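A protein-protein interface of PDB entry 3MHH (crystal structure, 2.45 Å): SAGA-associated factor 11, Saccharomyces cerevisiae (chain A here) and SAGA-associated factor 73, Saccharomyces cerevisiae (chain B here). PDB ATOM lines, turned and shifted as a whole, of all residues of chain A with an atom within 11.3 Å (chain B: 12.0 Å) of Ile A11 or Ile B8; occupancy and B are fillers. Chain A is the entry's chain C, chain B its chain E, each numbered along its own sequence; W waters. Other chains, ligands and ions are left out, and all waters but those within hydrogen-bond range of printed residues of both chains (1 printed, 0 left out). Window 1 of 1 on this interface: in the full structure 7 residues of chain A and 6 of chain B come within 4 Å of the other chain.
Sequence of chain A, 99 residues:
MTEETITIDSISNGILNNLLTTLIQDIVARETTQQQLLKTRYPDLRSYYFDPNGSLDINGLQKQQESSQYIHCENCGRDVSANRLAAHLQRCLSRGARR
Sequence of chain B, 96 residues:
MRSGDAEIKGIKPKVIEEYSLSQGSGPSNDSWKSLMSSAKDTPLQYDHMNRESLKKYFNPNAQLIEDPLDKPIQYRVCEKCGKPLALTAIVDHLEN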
ATOM      1  N   GLU A   4      23.052  -7.065  11.293  1.00  0.00           N
ATOM      2  CA  GLU A   4      23.670  -7.359  12.583  1.00  0.00           C
ATOM      3  C   GLU A   4      23.274  -8.770  13.011  1.00  0.00           C
ATOM      4  O   GLU A   4      22.247  -9.295  12.571  1.00  0.00           O
ATOM      5  CB  GLU A   4      23.241  -6.336  13.642  1.00  0.00           C
ATOM      6  CG  GLU A   4      23.592  -4.891  13.289  1.00  0.00           C
ATOM      7  CD  GLU A   4      22.675  -4.308  12.224  1.00  0.00           C
ATOM      8  OE1 GLU A   4      23.160  -4.046  11.098  1.00  0.00           O
ATOM      9  OE2 GLU A   4      21.468  -4.133  12.507  1.00  0.00           O
ATOM     10  N   THR A   5      24.104  -9.384  13.849  1.00  0.00           N
ATOM     11  CA  THR A   5      23.872 -10.753  14.299  1.00  0.00           C
ATOM     12  C   THR A   5      22.948 -10.755  15.519  1.00  0.00           C
ATOM     13  O   THR A   5      23.374 -10.478  16.639  1.00  0.00           O
ATOM     14  CB  THR A   5      25.198 -11.460  14.639  1.00  0.00           C
ATOM     15  OG1 THR A   5      26.142 -11.246  13.581  1.00  0.00           O
ATOM     16  CG2 THR A   5      24.975 -12.956  14.824  1.00  0.00           C
ATOM     17  N   ILE A   6      21.680 -11.078  15.292  1.00  0.00           N
ATOM     18  CA  ILE A   6      20.658 -10.948  16.322  1.00  0.00           C
ATOM     19  C   ILE A   6      20.858 -11.915  17.499  1.00  0.00           C
ATOM     20  O   ILE A   6      21.047 -13.122  17.313  1.00  0.00           O
ATOM     21  CB  ILE A   6      19.253 -11.080  15.714  1.00  0.00           C
ATOM     22  CG1 ILE A   6      19.024 -12.484  15.162  1.00  0.00           C
ATOM     23  CG2 ILE A   6      19.078 -10.063  14.587  1.00  0.00           C
ATOM     24  CD1 ILE A   6      17.853 -12.545  14.188  1.00  0.00           C
ATOM     25  N   THR A   7      20.847 -11.357  18.708  1.00  0.00           N
ATOM     26  CA  THR A   7      21.099 -12.126  19.923  1.00  0.00           C
ATOM     27  C   THR A   7      19.998 -11.893  20.949  1.00  0.00           C
ATOM     28  O   THR A   7      19.127 -11.032  20.762  1.00  0.00           O
ATOM     29  CB  THR A   7      22.424 -11.707  20.585  1.00  0.00           C
ATOM     30  OG1 THR A   7      22.301 -10.377  21.103  1.00  0.00           O
ATOM     31  CG2 THR A   7      23.590 -11.774  19.589  1.00  0.00           C
ATOM     32  N   ILE A   8      20.058 -12.640  22.048  1.00  0.00           N
ATOM     33  CA  ILE A   8      19.086 -12.473  23.119  1.00  0.00           C
ATOM     34  C   ILE A   8      19.139 -11.054  23.630  1.00  0.00           C
ATOM     35  O   ILE A   8      18.117 -10.497  24.012  1.00  0.00           O
ATOM     36  CB  ILE A   8      19.317 -13.429  24.303  1.00  0.00           C
ATOM     37  CG1 ILE A   8      18.956 -14.857  23.918  1.00  0.00           C
ATOM     38  CG2 ILE A   8      18.432 -13.031  25.486  1.00  0.00           C
ATOM     39  CD1 ILE A   8      19.029 -15.839  25.085  1.00  0.00           C
ATOM     40  N   ASP A   9      20.337 -10.467  23.632  1.00  0.00           N
ATOM     41  CA  ASP A   9      20.501  -9.075  24.063  1.00  0.00           C
ATOM     42  C   ASP A   9      19.842  -8.090  23.112  1.00  0.00           C
ATOM     43  O   ASP A   9      19.199  -7.148  23.552  1.00  0.00           O
ATOM     44  CB  ASP A   9      21.974  -8.712  24.241  1.00  0.00           C
ATOM     45  CG  ASP A   9      22.511  -9.106  25.606  1.00  0.00           C
ATOM     46  OD1 ASP A   9      23.728  -9.372  25.718  1.00  0.00           O
ATOM     47  OD2 ASP A   9      21.715  -9.155  26.566  1.00  0.00           O
ATOM     48  N   SER A  10      20.000  -8.308  21.813  1.00  0.00           N
ATOM     49  CA  SER A  10      19.450  -7.388  20.829  1.00  0.00           C
ATOM     50  C   SER A  10      17.936  -7.525  20.777  1.00  0.00           C
ATOM     51  O   SER A  10      17.220  -6.532  20.673  1.00  0.00           O
ATOM     52  CB  SER A  10      20.068  -7.625  19.440  1.00  0.00           C
ATOM     53  OG  SER A  10      19.454  -8.699  18.750  1.00  0.00           O
ATOM     54  N   ILE A  11      17.437  -8.749  20.856  1.00  0.00           N
ATOM     55  CA  ILE A  11      15.999  -8.939  20.886  1.00  0.00           C
ATOM     56  C   ILE A  11      15.443  -8.250  22.125  1.00  0.00           C
ATOM     57  O   ILE A  11      14.437  -7.541  22.044  1.00  0.00           O
ATOM     58  CB  ILE A  11      15.591 -10.426  20.903  1.00  0.00           C
ATOM     59  CG1 ILE A  11      15.900 -11.072  19.553  1.00  0.00           C
ATOM     60  CG2 ILE A  11      14.111 -10.562  21.190  1.00  0.00           C
ATOM     61  CD1 ILE A  11      15.234 -10.362  18.382  1.00  0.00           C
ATOM     62  N   SER A  12      16.117  -8.449  23.255  1.00  0.00           N
ATOM     63  CA  SER A  12      15.697  -7.872  24.522  1.00  0.00           C
ATOM     64  C   SER A  12      15.699  -6.354  24.513  1.00  0.00           C
ATOM     65  O   SER A  12      14.734  -5.733  24.953  1.00  0.00           O
ATOM     66  CB  SER A  12      16.557  -8.393  25.669  1.00  0.00           C
ATOM     67  OG  SER A  12      16.143  -9.698  26.038  1.00  0.00           O
ATOM     68  N   ASN A  13      16.761  -5.743  24.006  1.00  0.00           N
ATOM     69  CA  ASN A  13      16.761  -4.293  23.871  1.00  0.00           C
ATOM     70  C   ASN A  13      15.583  -3.875  22.991  1.00  0.00           C
ATOM     71  O   ASN A  13      14.875  -2.915  23.293  1.00  0.00           O
ATOM     72  CB  ASN A  13      18.084  -3.785  23.302  1.00  0.00           C
ATOM     73  CG  ASN A  13      19.201  -3.772  24.340  1.00  0.00           C
ATOM     74  OD1 ASN A  13      19.195  -2.958  25.267  1.00  0.00           O
ATOM     75  ND2 ASN A  13      20.175  -4.666  24.181  1.00  0.00           N
ATOM     76  N   GLY A  14      15.342  -4.639  21.931  1.00  0.00           N
ATOM     77  CA  GLY A  14      14.226  -4.357  21.034  1.00  0.00           C
ATOM     78  C   GLY A  14      12.889  -4.409  21.750  1.00  0.00           C
ATOM     79  O   GLY A  14      12.016  -3.570  21.514  1.00  0.00           O
ATOM     80  N   ILE A  15      12.722  -5.403  22.618  1.00  0.00           N
ATOM     81  CA  ILE A  15      11.493  -5.528  23.404  1.00  0.00           C
ATOM     82  C   ILE A  15      11.366  -4.357  24.378  1.00  0.00           C
ATOM     83  O   ILE A  15      10.314  -3.750  24.473  1.00  0.00           O
ATOM     84  CB  ILE A  15      11.441  -6.863  24.156  1.00  0.00           C
ATOM     85  CG1 ILE A  15      11.302  -8.009  23.158  1.00  0.00           C
ATOM     86  CG2 ILE A  15      10.290  -6.901  25.165  1.00  0.00           C
ATOM     87  CD1 ILE A  15      11.433  -9.365  23.799  1.00  0.00           C
ATOM     88  N   LEU A  16      12.450  -4.010  25.058  1.00  0.00           N
ATOM     89  CA  LEU A  16      12.425  -2.907  25.995  1.00  0.00           C
ATOM     90  C   LEU A  16      12.102  -1.598  25.293  1.00  0.00           C
ATOM     91  O   LEU A  16      11.366  -0.768  25.830  1.00  0.00           O
ATOM     92  CB  LEU A  16      13.765  -2.782  26.735  1.00  0.00           C
ATOM     93  CG  LEU A  16      13.803  -1.628  27.750  1.00  0.00           C
ATOM     94  CD1 LEU A  16      12.819  -1.898  28.856  1.00  0.00           C
ATOM     95  CD2 LEU A  16      15.215  -1.375  28.317  1.00  0.00           C
ATOM     96  N   ASN A  17      12.664  -1.419  24.099  1.00  0.00           N
ATOM     97  CA  ASN A  17      12.496  -0.190  23.312  1.00  0.00           C
ATOM     98  C   ASN A  17      11.041  -0.014  22.856  1.00  0.00           C
ATOM     99  O   ASN A  17      10.467   1.076  22.949  1.00  0.00           O
ATOM    100  CB  ASN A  17      13.449  -0.242  22.112  1.00  0.00           C
ATOM    101  CG  ASN A  17      13.384   1.004  21.234  1.00  0.00           C
ATOM    102  OD1 ASN A  17      12.889   0.940  20.107  1.00  0.00           O
ATOM    103  ND2 ASN A  17      13.920   2.125  21.724  1.00  0.00           N
ATOM    104  N   ASN A  18      10.434  -1.099  22.388  1.00  0.00           N
ATOM    105  CA  ASN A  18       9.002  -1.097  22.107  1.00  0.00           C
ATOM    106  C   ASN A  18       8.230  -0.649  23.355  1.00  0.00           C
ATOM    107  O   ASN A  18       7.381   0.252  23.286  1.00  0.00           O
ATOM    108  CB  ASN A  18       8.518  -2.488  21.674  1.00  0.00           C
ATOM    109  CG  ASN A  18       8.825  -2.800  20.202  1.00  0.00           C
ATOM    110  OD1 ASN A  18       8.179  -3.651  19.588  1.00  0.00           O
ATOM    111  ND2 ASN A  18       9.805  -2.123  19.644  1.00  0.00           N
ATOM    112  N   LEU A  19       8.536  -1.261  24.496  1.00  0.00           N
ATOM    113  CA  LEU A  19       7.818  -0.930  25.721  1.00  0.00           C
ATOM    114  C   LEU A  19       8.073   0.529  26.036  1.00  0.00           C
ATOM    115  O   LEU A  19       7.148   1.285  26.369  1.00  0.00           O
ATOM    116  CB  LEU A  19       8.266  -1.815  26.886  1.00  0.00           C
ATOM    117  CG  LEU A  19       7.741  -3.254  26.932  1.00  0.00           C
ATOM    118  CD1 LEU A  19       8.592  -4.125  27.854  1.00  0.00           C
ATOM    119  CD2 LEU A  19       6.271  -3.315  27.356  1.00  0.00           C
ATOM    120  N   LEU A  20       9.331   0.939  25.903  1.00  0.00           N
ATOM    121  CA  LEU A  20       9.708   2.300  26.268  1.00  0.00           C
ATOM    122  C   LEU A  20       9.071   3.338  25.340  1.00  0.00           C
ATOM    123  O   LEU A  20       8.494   4.309  25.809  1.00  0.00           O
ATOM    124  CB  LEU A  20      11.229   2.447  26.310  1.00  0.00           C
ATOM    125  CG  LEU A  20      11.914   1.906  27.565  1.00  0.00           C
ATOM    126  CD1 LEU A  20      13.436   1.972  27.428  1.00  0.00           C
ATOM    127  CD2 LEU A  20      11.459   2.672  28.798  1.00  0.00           C
ATOM    128  N   ASP B   5      28.160 -11.615  22.391  1.00  0.00           N
ATOM    129  CA  ASP B   5      27.475 -12.726  23.113  1.00  0.00           C
ATOM    130  C   ASP B   5      26.876 -13.710  22.105  1.00  0.00           C
ATOM    131  O   ASP B   5      27.186 -13.644  20.911  1.00  0.00           O
ATOM    132  CB  ASP B   5      26.392 -12.171  24.050  1.00  0.00           C
ATOM    133  CG  ASP B   5      26.505 -12.723  25.469  1.00  0.00           C
ATOM    134  OD1 ASP B   5      25.527 -13.333  25.955  1.00  0.00           O
ATOM    135  OD2 ASP B   5      27.579 -12.551  26.093  1.00  0.00           O
ATOM    136  N   ALA B   6      26.015 -14.609  22.582  1.00  0.00           N
ATOM    137  CA  ALA B   6      25.565 -15.754  21.775  1.00  0.00           C
ATOM    138  C   ALA B   6      24.467 -15.425  20.757  1.00  0.00           C
ATOM    139  O   ALA B   6      23.456 -14.793  21.084  1.00  0.00           O
ATOM    140  CB  ALA B   6      25.113 -16.898  22.685  1.00  0.00           C
ATOM    141  N   GLU B   7      24.675 -15.890  19.527  1.00  0.00           N
ATOM    142  CA  GLU B   7      23.720 -15.713  18.438  1.00  0.00           C
ATOM    143  C   GLU B   7      22.528 -16.640  18.641  1.00  0.00           C
ATOM    144  O   GLU B   7      22.679 -17.750  19.149  1.00  0.00           O
ATOM    145  CB  GLU B   7      24.403 -16.035  17.105  1.00  0.00           C
ATOM    146  CG  GLU B   7      23.529 -15.869  15.870  1.00  0.00           C
ATOM    147  CD  GLU B   7      24.306 -16.088  14.576  1.00  0.00           C
ATOM    148  OE1 GLU B   7      25.257 -16.902  14.569  1.00  0.00           O
ATOM    149  OE2 GLU B   7      23.962 -15.449  13.562  1.00  0.00           O
ATOM    150  N   ILE B   8      21.345 -16.182  18.241  1.00  0.00           N
ATOM    151  CA  ILE B   8      20.136 -16.994  18.368  1.00  0.00           C
ATOM    152  C   ILE B   8      19.929 -17.917  17.166  1.00  0.00           C
ATOM    153  O   ILE B   8      19.929 -17.461  16.029  1.00  0.00           O
ATOM    154  CB  ILE B   8      18.891 -16.112  18.526  1.00  0.00           C
ATOM    155  CG1 ILE B   8      18.946 -15.363  19.856  1.00  0.00           C
ATOM    156  CG2 ILE B   8      17.633 -16.965  18.470  1.00  0.00           C
ATOM    157  CD1 ILE B   8      17.886 -14.295  20.002  1.00  0.00           C
ATOM    158  N   LYS B   9      19.760 -19.211  17.419  1.00  0.00           N
ATOM    159  CA  LYS B   9      19.423 -20.159  16.357  1.00  0.00           C
ATOM    160  C   LYS B   9      17.968 -19.983  15.952  1.00  0.00           C
ATOM    161  O   LYS B   9      17.634 -19.869  14.778  1.00  0.00           O
ATOM    162  CB  LYS B   9      19.637 -21.604  16.816  1.00  0.00           C
ATOM    163  CG  LYS B   9      18.950 -22.629  15.908  1.00  0.00           C
ATOM    164  CD  LYS B   9      19.200 -24.084  16.330  1.00  0.00           C
ATOM    165  CE  LYS B   9      18.459 -24.461  17.622  1.00  0.00           C
ATOM    166  NZ  LYS B   9      16.999 -24.102  17.643  1.00  0.00           N
ATOM    167  N   GLY B  10      17.101 -19.980  16.949  1.00  0.00           N
ATOM    168  CA  GLY B  10      15.673 -19.879  16.727  1.00  0.00           C
ATOM    169  C   GLY B  10      14.996 -20.059  18.061  1.00  0.00           C
ATOM    170  O   GLY B  10      15.660 -20.209  19.087  1.00  0.00           O
ATOM    171  N   ILE B  11      13.674 -20.027  18.058  1.00  0.00           N
ATOM    172  CA  ILE B  11      12.941 -20.319  19.266  1.00  0.00           C
ATOM    173  C   ILE B  11      12.735 -21.822  19.375  1.00  0.00           C
ATOM    174  O   ILE B  11      12.541 -22.514  18.368  1.00  0.00           O
ATOM    175  CB  ILE B  11      11.603 -19.548  19.335  1.00  0.00           C
ATOM    176  CG1 ILE B  11      10.632 -20.259  20.277  1.00  0.00           C
ATOM    177  CG2 ILE B  11      10.997 -19.387  17.945  1.00  0.00           C
ATOM    178  CD1 ILE B  11       9.390 -19.471  20.546  1.00  0.00           C
ATOM    179  N   LYS B  12      12.822 -22.332  20.600  1.00  0.00           N
ATOM    180  CA  LYS B  12      12.645 -23.754  20.829  1.00  0.00           C
ATOM    181  C   LYS B  12      11.428 -24.259  20.071  1.00  0.00           C
ATOM    182  O   LYS B  12      10.327 -23.716  20.209  1.00  0.00           O
ATOM    183  CB  LYS B  12      12.510 -24.064  22.321  1.00  0.00           C
ATOM    184  CG  LYS B  12      13.819 -23.963  23.080  1.00  0.00           C
ATOM    185  CD  LYS B  12      13.651 -24.253  24.557  1.00  0.00           C
ATOM    186  CE  LYS B  12      14.999 -24.520  25.215  1.00  0.00           C
ATOM    187  NZ  LYS B  12      16.023 -23.516  24.817  1.00  0.00           N
ATOM    188  N   PRO B  13      11.632 -25.294  19.248  1.00  0.00           N
ATOM    189  CA  PRO B  13      10.540 -25.945  18.557  1.00  0.00           C
ATOM    190  C   PRO B  13       9.406 -26.278  19.513  1.00  0.00           C
ATOM    191  O   PRO B  13       8.246 -26.046  19.195  1.00  0.00           O
ATOM    192  CB  PRO B  13      11.181 -27.225  18.019  1.00  0.00           C
ATOM    193  CG  PRO B  13      12.632 -26.890  17.868  1.00  0.00           C
ATOM    194  CD  PRO B  13      12.934 -25.937  18.974  1.00  0.00           C
ATOM    195  N   VAL B  15       8.476 -24.871  22.148  1.00  0.00           N
ATOM    196  CA  VAL B  15       7.754 -23.651  22.486  1.00  0.00           C
ATOM    197  C   VAL B  15       6.928 -23.164  21.301  1.00  0.00           C
ATOM    198  O   VAL B  15       5.797 -22.708  21.466  1.00  0.00           O
ATOM    199  CB  VAL B  15       8.713 -22.534  22.916  1.00  0.00           C
ATOM    200  CG1 VAL B  15       7.939 -21.243  23.183  1.00  0.00           C
ATOM    201  CG2 VAL B  15       9.499 -22.956  24.149  1.00  0.00           C
ATOM    202  N   ILE B  16       7.490 -23.265  20.099  1.00  0.00           N
ATOM    203  CA  ILE B  16       6.747 -22.908  18.895  1.00  0.00           C
ATOM    204  C   ILE B  16       5.414 -23.640  18.868  1.00  0.00           C
ATOM    205  O   ILE B  16       4.385 -23.042  18.557  1.00  0.00           O
ATOM    206  CB  ILE B  16       7.530 -23.239  17.610  1.00  0.00           C
ATOM    207  CG1 ILE B  16       8.523 -22.123  17.285  1.00  0.00           C
ATOM    208  CG2 ILE B  16       6.585 -23.412  16.434  1.00  0.00           C
ATOM    209  CD1 ILE B  16       9.288 -22.353  16.010  1.00  0.00           C
ATOM    210  N   LEU B  21       3.035 -20.670  17.516  1.00  0.00           N
ATOM    211  CA  LEU B  21       3.727 -19.463  17.088  1.00  0.00           C
ATOM    212  C   LEU B  21       3.861 -19.325  15.566  1.00  0.00           C
ATOM    213  O   LEU B  21       3.875 -18.216  15.047  1.00  0.00           O
ATOM    214  CB  LEU B  21       5.106 -19.399  17.738  1.00  0.00           C
ATOM    215  CG  LEU B  21       5.237 -18.490  18.953  1.00  0.00           C
ATOM    216  CD1 LEU B  21       3.965 -18.456  19.797  1.00  0.00           C
ATOM    217  CD2 LEU B  21       6.437 -18.920  19.776  1.00  0.00           C
HETATM  218  O   HOH W   1      23.063 -12.032  24.276  1.00  0.00           O
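Water W1 bridges the side-chain carboxylate (OD1) of Asp A9 (3.1 Å) and the side-chain carboxylate (OD1) of Asp B5 (3.3 Å).
Ile A11 touches just one residue of chain B: Ile B8.
Of chain A, only Ile A6 (3.2 Å), Thr A7 (3.3 Å), Ile A8 (3.4 Å) and Ile A11 (3.8 Å) come within 4 Å of Ile B8.
Printed residues of chain B within 4 Å of Ile A6: Glu B7 and Ile B8.
Thr A7 touches just these residues of chain B: Ala B6 and Ile B8.
Of chain B, only Ile B8 (3.4 Å) comes within 4 Å of Ile A8.
No residue of chain B comes within 4 Å of Ser A10.
No residue of chain B comes within 4 Å of Ser A12.
No residue of chain B comes within 4 Å of Asn A13.
No residue of chain B comes within 4 Å of Gly A14.
No residue of chain B comes within 4 Å of Ile A15.
Ala B6 touches one residue of chain A.
Glu B7 touches two residues of chain A.
No residue of chain A comes within 4 Å of Lys B9.
No residue of chain A comes within 4 Å of Gly B10.
Printed residues of chain B within 4 Å of Thr A5: Glu B7.
Asp B5 touches none of the printed residues of chain A.
Asn A17 touches none of the printed residues of chain B.
The nearest residue of chain A that does not touch Ile B8 is Asp A9 (5.8 Å).
O of Ile A8 lies within hydrogen-bond range of OG of Ser A12 (2.9 Å).
The side-chain hydroxyl (OG) of Ser A10 sits at hydrogen-bond distance from the backbone NH (N) of Thr A7 (3.0 Å).
OG1 of Thr A7 sits close to N of Asp A9.
Printed residues of chain B that touch a printed residue of chain A: Ala B6, Glu B7 and Ile B8.
Hydrophobic or aromatic side chains of chain B that line the printed part of chain A: Ile B8.
N of Ile B8 lies within hydrogen-bond range of O of Ile A6 (3.2 Å).
Among the printed residues, pairs that only touch across the chains: Thr A5 with Glu B7, Thr A7 with Ala B6, Thr A7 with Ile B8, Ile A8 with Ile B8, Ile A11 with Ile B8 and Ile A6 with Glu B7.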
